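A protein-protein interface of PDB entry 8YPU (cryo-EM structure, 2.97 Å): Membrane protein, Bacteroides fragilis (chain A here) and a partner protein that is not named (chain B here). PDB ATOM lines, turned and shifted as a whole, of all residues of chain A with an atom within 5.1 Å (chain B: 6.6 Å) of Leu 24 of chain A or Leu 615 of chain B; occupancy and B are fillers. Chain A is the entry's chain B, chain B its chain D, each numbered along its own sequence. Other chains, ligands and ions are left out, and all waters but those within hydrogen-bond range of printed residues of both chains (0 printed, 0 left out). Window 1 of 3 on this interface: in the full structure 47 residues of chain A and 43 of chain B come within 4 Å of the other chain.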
ATOM      1  N   VAL A  13      22.070  -2.670   3.671  1.00  0.00           N
ATOM      2  CA  VAL A  13      22.584  -1.845   4.755  1.00  0.00           C
ATOM      3  C   VAL A  13      22.226  -2.537   6.060  1.00  0.00           C
ATOM      4  O   VAL A  13      21.052  -2.601   6.436  1.00  0.00           O
ATOM      5  CB  VAL A  13      22.012  -0.423   4.701  1.00  0.00           C
ATOM      6  CG1 VAL A  13      22.418   0.368   5.927  1.00  0.00           C
ATOM      7  CG2 VAL A  13      22.474   0.278   3.447  1.00  0.00           C
ATOM      8  N   ILE A  14      23.231  -3.063   6.753  1.00  0.00           N
ATOM      9  CA  ILE A  14      23.051  -3.664   8.072  1.00  0.00           C
ATOM     10  C   ILE A  14      23.580  -2.669   9.101  1.00  0.00           C
ATOM     11  O   ILE A  14      24.800  -2.451   9.162  1.00  0.00           O
ATOM     12  CB  ILE A  14      23.766  -5.016   8.190  1.00  0.00           C
ATOM     13  CG1 ILE A  14      23.206  -6.021   7.185  1.00  0.00           C
ATOM     14  CG2 ILE A  14      23.624  -5.565   9.593  1.00  0.00           C
ATOM     15  CD1 ILE A  14      24.178  -6.417   6.120  1.00  0.00           C
ATOM     16  N   PRO A  15      22.722  -2.051   9.915  1.00  0.00           N
ATOM     17  CA  PRO A  15      23.183  -1.010  10.845  1.00  0.00           C
ATOM     18  C   PRO A  15      24.100  -1.580  11.915  1.00  0.00           C
ATOM     19  O   PRO A  15      23.716  -2.478  12.665  1.00  0.00           O
ATOM     20  CB  PRO A  15      21.878  -0.474  11.449  1.00  0.00           C
ATOM     21  CG  PRO A  15      20.810  -0.913  10.522  1.00  0.00           C
ATOM     22  CD  PRO A  15      21.262  -2.204   9.947  1.00  0.00           C
ATOM     23  N   GLU A  20      24.537   4.668  11.828  1.00  0.00           N
ATOM     24  CA  GLU A  20      23.491   3.865  11.206  1.00  0.00           C
ATOM     25  C   GLU A  20      22.351   3.592  12.175  1.00  0.00           C
ATOM     26  O   GLU A  20      21.180   3.574  11.778  1.00  0.00           O
ATOM     27  CB  GLU A  20      24.086   2.566  10.675  1.00  0.00           C
ATOM     28  CG  GLU A  20      25.250   2.795   9.738  1.00  0.00           C
ATOM     29  CD  GLU A  20      25.724   1.531   9.065  1.00  0.00           C
ATOM     30  OE1 GLU A  20      26.534   0.801   9.669  1.00  0.00           O
ATOM     31  OE2 GLU A  20      25.289   1.268   7.928  1.00  0.00           O
ATOM     32  N   TYR A  21      22.662   3.388  13.453  1.00  0.00           N
ATOM     33  CA  TYR A  21      21.595   3.219  14.430  1.00  0.00           C
ATOM     34  C   TYR A  21      20.837   4.517  14.662  1.00  0.00           C
ATOM     35  O   TYR A  21      19.629   4.487  14.910  1.00  0.00           O
ATOM     36  CB  TYR A  21      22.155   2.666  15.735  1.00  0.00           C
ATOM     37  CG  TYR A  21      22.079   1.164  15.773  1.00  0.00           C
ATOM     38  CD1 TYR A  21      20.881   0.523  16.033  1.00  0.00           C
ATOM     39  CD2 TYR A  21      23.190   0.388  15.505  1.00  0.00           C
ATOM     40  CE1 TYR A  21      20.799  -0.844  16.051  1.00  0.00           C
ATOM     41  CE2 TYR A  21      23.117  -0.982  15.521  1.00  0.00           C
ATOM     42  CZ  TYR A  21      21.919  -1.592  15.795  1.00  0.00           C
ATOM     43  OH  TYR A  21      21.839  -2.962  15.809  1.00  0.00           O
ATOM     44  N   ARG A  22      21.510   5.665  14.557  1.00  0.00           N
ATOM     45  CA  ARG A  22      20.784   6.927  14.619  1.00  0.00           C
ATOM     46  C   ARG A  22      19.891   7.103  13.399  1.00  0.00           C
ATOM     47  O   ARG A  22      18.798   7.658  13.506  1.00  0.00           O
ATOM     48  CB  ARG A  22      21.748   8.102  14.742  1.00  0.00           C
ATOM     49  CG  ARG A  22      21.043   9.447  14.688  1.00  0.00           C
ATOM     50  CD  ARG A  22      21.567  10.413  15.735  1.00  0.00           C
ATOM     51  NE  ARG A  22      21.139  10.111  17.096  1.00  0.00           N
ATOM     52  CZ  ARG A  22      19.900  10.236  17.549  1.00  0.00           C
ATOM     53  NH1 ARG A  22      18.901  10.576  16.753  1.00  0.00           N
ATOM     54  NH2 ARG A  22      19.658  10.019  18.837  1.00  0.00           N
ATOM     55  N   ALA A  23      20.339   6.645  12.229  1.00  0.00           N
ATOM     56  CA  ALA A  23      19.482   6.686  11.045  1.00  0.00           C
ATOM     57  C   ALA A  23      18.249   5.805  11.225  1.00  0.00           C
ATOM     58  O   ALA A  23      17.130   6.199  10.868  1.00  0.00           O
ATOM     59  CB  ALA A  23      20.272   6.254   9.814  1.00  0.00           C
ATOM     60  N   LEU A  24      18.440   4.609  11.780  1.00  0.00           N
ATOM     61  CA  LEU A  24      17.318   3.716  12.060  1.00  0.00           C
ATOM     62  C   LEU A  24      16.345   4.342  13.058  1.00  0.00           C
ATOM     63  O   LEU A  24      15.125   4.295  12.866  1.00  0.00           O
ATOM     64  CB  LEU A  24      17.857   2.381  12.576  1.00  0.00           C
ATOM     65  CG  LEU A  24      17.018   1.103  12.572  1.00  0.00           C
ATOM     66  CD1 LEU A  24      16.989   0.480  11.200  1.00  0.00           C
ATOM     67  CD2 LEU A  24      17.579   0.125  13.582  1.00  0.00           C
ATOM     68  N   LEU A  25      16.871   4.950  14.124  1.00  0.00           N
ATOM     69  CA  LEU A  25      16.016   5.601  15.112  1.00  0.00           C
ATOM     70  C   LEU A  25      15.331   6.839  14.551  1.00  0.00           C
ATOM     71  O   LEU A  25      14.221   7.168  14.971  1.00  0.00           O
ATOM     72  CB  LEU A  25      16.829   5.960  16.352  1.00  0.00           C
ATOM     73  CG  LEU A  25      16.052   6.210  17.643  1.00  0.00           C
ATOM     74  CD1 LEU A  25      15.158   5.035  17.983  1.00  0.00           C
ATOM     75  CD2 LEU A  25      17.016   6.485  18.770  1.00  0.00           C
ATOM     76  N   ALA A  26      15.970   7.546  13.621  1.00  0.00           N
ATOM     77  CA  ALA A  26      15.316   8.672  12.965  1.00  0.00           C
ATOM     78  C   ALA A  26      14.152   8.203  12.105  1.00  0.00           C
ATOM     79  O   ALA A  26      13.091   8.837  12.080  1.00  0.00           O
ATOM     80  CB  ALA A  26      16.327   9.444  12.124  1.00  0.00           C
ATOM     81  N   ARG A  27      14.337   7.094  11.388  1.00  0.00           N
ATOM     82  CA  ARG A  27      13.227   6.503  10.647  1.00  0.00           C
ATOM     83  C   ARG A  27      12.103   6.086  11.588  1.00  0.00           C
ATOM     84  O   ARG A  27      10.923   6.225  11.255  1.00  0.00           O
ATOM     85  CB  ARG A  27      13.726   5.317   9.828  1.00  0.00           C
ATOM     86  CG  ARG A  27      12.641   4.407   9.306  1.00  0.00           C
ATOM     87  CD  ARG A  27      11.721   5.120   8.339  1.00  0.00           C
ATOM     88  NE  ARG A  27      12.445   5.669   7.202  1.00  0.00           N
ATOM     89  CZ  ARG A  27      11.868   6.270   6.171  1.00  0.00           C
ATOM     90  NH1 ARG A  27      10.554   6.396   6.095  1.00  0.00           N
ATOM     91  NH2 ARG A  27      12.626   6.751   5.192  1.00  0.00           N
ATOM     92  N   ALA A  28      12.452   5.569  12.768  1.00  0.00           N
ATOM     93  CA  ALA A  28      11.435   5.267  13.776  1.00  0.00           C
ATOM     94  C   ALA A  28      10.704   6.524  14.232  1.00  0.00           C
ATOM     95  O   ALA A  28       9.481   6.514  14.397  1.00  0.00           O
ATOM     96  CB  ALA A  28      12.072   4.569  14.973  1.00  0.00           C
ATOM     97  N   ILE A  87      11.584  -0.932  16.347  1.00  0.00           N
ATOM     98  CA  ILE A  87      12.872  -0.287  16.102  1.00  0.00           C
ATOM     99  C   ILE A  87      13.485   0.217  17.406  1.00  0.00           C
ATOM    100  O   ILE A  87      14.700   0.110  17.621  1.00  0.00           O
ATOM    101  CB  ILE A  87      12.731   0.835  15.064  1.00  0.00           C
ATOM    102  CG1 ILE A  87      12.322   0.244  13.720  1.00  0.00           C
ATOM    103  CG2 ILE A  87      14.038   1.573  14.916  1.00  0.00           C
ATOM    104  CD1 ILE A  87      11.546   1.191  12.858  1.00  0.00           C
ATOM    105  N   GLN A  90      14.955  -2.770  19.050  1.00  0.00           N
ATOM    106  CA  GLN A  90      16.190  -3.170  18.382  1.00  0.00           C
ATOM    107  C   GLN A  90      17.360  -2.313  18.844  1.00  0.00           C
ATOM    108  O   GLN A  90      18.445  -2.826  19.147  1.00  0.00           O
ATOM    109  CB  GLN A  90      16.012  -3.072  16.867  1.00  0.00           C
ATOM    110  CG  GLN A  90      17.273  -3.306  16.065  1.00  0.00           C
ATOM    111  CD  GLN A  90      17.579  -4.775  15.873  1.00  0.00           C
ATOM    112  OE1 GLN A  90      16.681  -5.608  15.847  1.00  0.00           O
ATOM    113  NE2 GLN A  90      18.855  -5.099  15.735  1.00  0.00           N
ATOM    114  N   VAL A  91      17.150  -0.998  18.916  1.00  0.00           N
ATOM    115  CA  VAL A  91      18.206  -0.104  19.387  1.00  0.00           C
ATOM    116  C   VAL A  91      18.553  -0.404  20.841  1.00  0.00           C
ATOM    117  O   VAL A  91      19.719  -0.339  21.241  1.00  0.00           O
ATOM    118  CB  VAL A  91      17.794   1.366  19.189  1.00  0.00           C
ATOM    119  CG1 VAL A  91      18.843   2.291  19.760  1.00  0.00           C
ATOM    120  CG2 VAL A  91      17.588   1.658  17.717  1.00  0.00           C
ATOM    121  N   SER B 612      18.335 -14.385   5.958  1.00  0.00           N
ATOM    122  CA  SER B 612      19.413 -13.840   6.764  1.00  0.00           C
ATOM    123  C   SER B 612      18.924 -13.520   8.168  1.00  0.00           C
ATOM    124  O   SER B 612      17.752 -13.186   8.363  1.00  0.00           O
ATOM    125  CB  SER B 612      19.978 -12.569   6.115  1.00  0.00           C
ATOM    126  OG  SER B 612      21.250 -12.239   6.631  1.00  0.00           O
ATOM    127  N   PRO B 613      19.798 -13.627   9.165  1.00  0.00           N
ATOM    128  CA  PRO B 613      19.452 -13.205  10.528  1.00  0.00           C
ATOM    129  C   PRO B 613      19.720 -11.737  10.820  1.00  0.00           C
ATOM    130  O   PRO B 613      19.688 -11.349  11.989  1.00  0.00           O
ATOM    131  CB  PRO B 613      20.370 -14.086  11.391  1.00  0.00           C
ATOM    132  CG  PRO B 613      21.207 -14.887  10.443  1.00  0.00           C
ATOM    133  CD  PRO B 613      21.130 -14.236   9.123  1.00  0.00           C
ATOM    134  N   PHE B 614      19.987 -10.930   9.802  1.00  0.00           N
ATOM    135  CA  PHE B 614      20.454  -9.568   9.975  1.00  0.00           C
ATOM    136  C   PHE B 614      19.378  -8.577   9.569  1.00  0.00           C
ATOM    137  O   PHE B 614      18.447  -8.899   8.829  1.00  0.00           O
ATOM    138  CB  PHE B 614      21.720  -9.317   9.152  1.00  0.00           C
ATOM    139  CG  PHE B 614      22.923 -10.045   9.658  1.00  0.00           C
ATOM    140  CD1 PHE B 614      23.597  -9.598  10.773  1.00  0.00           C
ATOM    141  CD2 PHE B 614      23.388 -11.169   9.013  1.00  0.00           C
ATOM    142  CE1 PHE B 614      24.703 -10.264  11.236  1.00  0.00           C
ATOM    143  CE2 PHE B 614      24.490 -11.839   9.477  1.00  0.00           C
ATOM    144  CZ  PHE B 614      25.149 -11.383  10.586  1.00  0.00           C
ATOM    145  N   LEU B 615      19.525  -7.355  10.069  1.00  0.00           N
ATOM    146  CA  LEU B 615      18.640  -6.253   9.715  1.00  0.00           C
ATOM    147  C   LEU B 615      19.087  -5.723   8.363  1.00  0.00           C
ATOM    148  O   LEU B 615      20.049  -4.963   8.268  1.00  0.00           O
ATOM    149  CB  LEU B 615      18.680  -5.170  10.788  1.00  0.00           C
ATOM    150  CG  LEU B 615      17.813  -3.922  10.634  1.00  0.00           C
ATOM    151  CD1 LEU B 615      16.482  -4.295  10.093  1.00  0.00           C
ATOM    152  CD2 LEU B 615      17.640  -3.251  11.972  1.00  0.00           C
ATOM    153  N   LEU B 616      18.403  -6.145   7.308  1.00  0.00           N
ATOM    154  CA  LEU B 616      18.676  -5.662   5.963  1.00  0.00           C
ATOM    155  C   LEU B 616      17.787  -4.458   5.691  1.00  0.00           C
ATOM    156  O   LEU B 616      16.558  -4.582   5.675  1.00  0.00           O
ATOM    157  CB  LEU B 616      18.428  -6.761   4.934  1.00  0.00           C
ATOM    158  CG  LEU B 616      19.067  -8.116   5.229  1.00  0.00           C
ATOM    159  CD1 LEU B 616      18.514  -9.159   4.293  1.00  0.00           C
ATOM    160  CD2 LEU B 616      20.575  -8.035   5.107  1.00  0.00           C
ATOM    161  N   GLY B 617      18.404  -3.301   5.486  1.00  0.00           N
ATOM    162  CA  GLY B 617      17.662  -2.078   5.271  1.00  0.00           C
ATOM    163  C   GLY B 617      18.110  -1.307   4.050  1.00  0.00           C
ATOM    164  O   GLY B 617      18.836  -1.835   3.207  1.00  0.00           O
ATOM    165  N   HIS B 631      19.879  11.240   6.572  1.00  0.00           N
ATOM    166  CA  HIS B 631      19.748   9.868   6.113  1.00  0.00           C
ATOM    167  C   HIS B 631      19.006   9.036   7.145  1.00  0.00           C
ATOM    168  O   HIS B 631      19.229   9.166   8.350  1.00  0.00           O
ATOM    169  CB  HIS B 631      21.122   9.261   5.846  1.00  0.00           C
ATOM    170  CG  HIS B 631      21.797   9.807   4.630  1.00  0.00           C
ATOM    171  ND1 HIS B 631      21.571   9.308   3.366  1.00  0.00           N
ATOM    172  CD2 HIS B 631      22.686  10.818   4.482  1.00  0.00           C
ATOM    173  CE1 HIS B 631      22.296   9.982   2.492  1.00  0.00           C
ATOM    174  NE2 HIS B 631      22.980  10.906   3.142  1.00  0.00           N
ATOM    175  N   MET B 632      18.110   8.184   6.663  1.00  0.00           N
ATOM    176  CA  MET B 632      17.357   7.272   7.504  1.00  0.00           C
ATOM    177  C   MET B 632      17.407   5.885   6.886  1.00  0.00           C
ATOM    178  O   MET B 632      17.537   5.741   5.670  1.00  0.00           O
ATOM    179  CB  MET B 632      15.902   7.718   7.661  1.00  0.00           C
ATOM    180  CG  MET B 632      15.725   9.210   7.820  1.00  0.00           C
ATOM    181  SD  MET B 632      13.997   9.688   7.817  1.00  0.00           S
ATOM    182  CE  MET B 632      13.946  10.727   9.263  1.00  0.00           C
ATOM    183  N   ILE B 633      17.298   4.864   7.728  1.00  0.00           N
ATOM    184  CA  ILE B 633      17.331   3.476   7.287  1.00  0.00           C
ATOM    185  C   ILE B 633      15.925   2.911   7.390  1.00  0.00           C
ATOM    186  O   ILE B 633      15.327   2.907   8.471  1.00  0.00           O
ATOM    187  CB  ILE B 633      18.324   2.636   8.105  1.00  0.00           C
ATOM    188  CG1 ILE B 633      19.754   3.082   7.837  1.00  0.00           C
ATOM    189  CG2 ILE B 633      18.186   1.170   7.765  1.00  0.00           C
ATOM    190  CD1 ILE B 633      20.770   2.369   8.674  1.00  0.00           C
ATOM    191  N   ASP B 634      15.399   2.438   6.267  1.00  0.00           N
ATOM    192  CA  ASP B 634      14.114   1.761   6.220  1.00  0.00           C
ATOM    193  C   ASP B 634      14.356   0.259   6.192  1.00  0.00           C
ATOM    194  O   ASP B 634      15.164  -0.226   5.397  1.00  0.00           O
ATOM    195  CB  ASP B 634      13.316   2.198   4.994  1.00  0.00           C
ATOM    196  CG  ASP B 634      11.822   2.216   5.246  1.00  0.00           C
ATOM    197  OD1 ASP B 634      11.387   1.745   6.317  1.00  0.00           O
ATOM    198  OD2 ASP B 634      11.078   2.702   4.369  1.00  0.00           O
ATOM    199  N   ILE B 635      13.656  -0.470   7.052  1.00  0.00           N
ATOM    200  CA  ILE B 635      13.876  -1.904   7.207  1.00  0.00           C
ATOM    201  C   ILE B 635      13.255  -2.641   6.028  1.00  0.00           C
ATOM    202  O   ILE B 635      12.052  -2.530   5.779  1.00  0.00           O
ATOM    203  CB  ILE B 635      13.288  -2.403   8.533  1.00  0.00           C
ATOM    204  CG1 ILE B 635      14.013  -1.761   9.714  1.00  0.00           C
ATOM    205  CG2 ILE B 635      13.339  -3.907   8.608  1.00  0.00           C
ATOM    206  CD1 ILE B 635      13.436  -2.141  11.053  1.00  0.00           C
ATOM    207  N   ASN B 636      14.074  -3.403   5.305  1.00  0.00           N
ATOM    208  CA  ASN B 636      13.571  -4.275   4.251  1.00  0.00           C
ATOM    209  C   ASN B 636      13.268  -5.673   4.766  1.00  0.00           C
ATOM    210  O   ASN B 636      12.261  -6.270   4.377  1.00  0.00           O
ATOM    211  CB  ASN B 636      14.574  -4.364   3.098  1.00  0.00           C
ATOM    212  CG  ASN B 636      14.621  -3.109   2.265  1.00  0.00           C
ATOM    213  OD1 ASN B 636      13.590  -2.578   1.866  1.00  0.00           O
ATOM    214  ND2 ASN B 636      15.823  -2.636   1.980  1.00  0.00           N
ATOM    215  N   SER B 637      14.124  -6.209   5.631  1.00  0.00           N
ATOM    216  CA  SER B 637      13.926  -7.526   6.215  1.00  0.00           C
ATOM    217  C   SER B 637      14.097  -7.450   7.722  1.00  0.00           C
ATOM    218  O   SER B 637      14.968  -6.736   8.222  1.00  0.00           O
ATOM    219  CB  SER B 637      14.900  -8.549   5.635  1.00  0.00           C
ATOM    220  OG  SER B 637      14.722  -8.686   4.238  1.00  0.00           O
ATOM    221  N   ALA B 638      13.269  -8.192   8.435  1.00  0.00           N
ATOM    222  CA  ALA B 638      13.305  -8.208   9.887  1.00  0.00           C
ATOM    223  C   ALA B 638      14.507  -9.005  10.391  1.00  0.00           C
ATOM    224  O   ALA B 638      14.889 -10.008   9.785  1.00  0.00           O
ATOM    225  CB  ALA B 638      12.022  -8.807  10.442  1.00  0.00           C
ATOM    226  N   PRO B 639      15.112  -8.579  11.492  1.00  0.00           N
ATOM    227  CA  PRO B 639      16.230  -9.326  12.080  1.00  0.00           C
ATOM    228  C   PRO B 639      15.799 -10.566  12.846  1.00  0.00           C
ATOM    229  O   PRO B 639      15.553 -10.487  14.052  1.00  0.00           O
ATOM    230  CB  PRO B 639      16.875  -8.303  13.024  1.00  0.00           C
ATOM    231  CG  PRO B 639      16.255  -6.996  12.690  1.00  0.00           C
ATOM    232  CD  PRO B 639      14.913  -7.287  12.155  1.00  0.00           C
ATOM    233  N   ASN B 640      15.671 -11.702  12.173  1.00  0.00           N
ATOM    234  CA  ASN B 640      15.322 -12.943  12.859  1.00  0.00           C
ATOM    235  C   ASN B 640      16.536 -13.453  13.620  1.00  0.00           C
ATOM    236  O   ASN B 640      17.445 -14.047  13.040  1.00  0.00           O
ATOM    237  CB  ASN B 640      14.822 -13.986  11.868  1.00  0.00           C
ATOM    238  CG  ASN B 640      13.945 -15.021  12.520  1.00  0.00           C
ATOM    239  OD1 ASN B 640      13.475 -14.833  13.637  1.00  0.00           O
ATOM    240  ND2 ASN B 640      13.719 -16.125  11.829  1.00  0.00           N
ATOM    241  N   PHE B 690       6.009  -5.993  11.872  1.00  0.00           N
ATOM    242  CA  PHE B 690       5.873  -6.359  10.472  1.00  0.00           C
ATOM    243  C   PHE B 690       4.590  -7.133  10.230  1.00  0.00           C
ATOM    244  O   PHE B 690       4.048  -7.780  11.130  1.00  0.00           O
ATOM    245  CB  PHE B 690       7.083  -7.173  10.014  1.00  0.00           C
ATOM    246  CG  PHE B 690       8.386  -6.515  10.328  1.00  0.00           C
ATOM    247  CD1 PHE B 690       8.949  -5.622   9.439  1.00  0.00           C
ATOM    248  CD2 PHE B 690       9.028  -6.756  11.520  1.00  0.00           C
ATOM    249  CE1 PHE B 690      10.130  -4.999   9.727  1.00  0.00           C
ATOM    250  CE2 PHE B 690      10.207  -6.134  11.810  1.00  0.00           C
ATOM    251  CZ  PHE B 690      10.761  -5.256  10.913  1.00  0.00           C
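Of the printed residues of chain B, Ala 23 of chain A touches His 631 (3.4 Å), Met 632 (3.5 Å) and Ile 633 (3.4 Å).
Of the printed residues of chain B, Leu 24 of chain A touches Leu 615 and Ile 633.
Leu 615 of chain B touches just these residues of chain A: Val 13 (3.2 Å), Ile 14 (3.3 Å), Pro 15 (3.4 Å) and Leu 24 (3.7 Å).
Of the printed residues of chain A, Leu 616 of chain B touches Val 13 and Ile 14.
Of the printed residues of chain A, His 631 of chain B touches Ala 23.
Of the printed residues of chain A, Ile 633 of chain B touches Val 13, Pro 15, Glu 20, Ala 23, Leu 24 and Arg 27.
Asn 640 of chain B touches none of the printed residues of chain A.
Of the 15 printed residues of chain A, 10 touch a printed residue of chain B.
Along chain A the printed residues that touch a printed residue of chain B span positions 13 to 90.
Of the 17 printed residues of chain B, 9 touch a printed residue of chain A.
Hydrophobic or aromatic side chains of chain B that line the printed part of chain A: Leu 615, Leu 616, Met 632, Ile 633, Ile 635 and Pro 639.
Among the printed residues, pairs that only touch across the chains: Val 13 of chain A with Leu 616 of chain B, Val 13 of chain A with Ile 633 of chain B, Ile 14 of chain A with Leu 615 of chain B, Ile 14 of chain A with Leu 616 of chain B, Pro 15 of chain A with Leu 615 of chain B, Pro 15 of chain A with Ile 633 of chain B, Glu 20 of chain A with Ile 633 of chain B, Ala 23 of chain A with His 631 of chain B, Ala 23 of chain A with Met 632 of chain B, Leu 24 of chain A with Leu 615 of chain B, Leu 24 of chain A with Ile 633 of chain B, Ala 26 of chain A with Met 632 of chain B, Arg 27 of chain A with Met 632 of chain B, Arg 27 of chain A with Ile 633 of chain B, Arg 27 of chain A with Asp 634 of chain B, Ile 87 of chain A with Ile 635 of chain B and Gln 90 of chain A with Pro 639 of chain B.
The backbone carbonyl oxygen (O) of Leu 616 of chain B lies within hydrogen-bond range of the backbone NH (N) of Asn 636 of chain B.
O of Leu 616 of chain B is in hydrogen-bond range of N of Ser 637 of chain B (2.9 Å).
The backbone carbonyl oxygen (O) of Gly 617 of chain B sits at hydrogen-bond distance from the side-chain amide nitrogen (ND2) of Asn 636 of chain B (3.4 Å).
The backbone carbonyl oxygen (O) of Val 13 of chain A lies within hydrogen-bond range of the backbone NH (N) of Gly 617 of chain B (2.9 Å).
The backbone carbonyl oxygen of Ala 23 of chain A sits at hydrogen-bond distance from the backbone NH of Ile 633 of chain B.
O of Leu 615 of chain B lies close to O of Val 13 of chain A, at 3.2 Å.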
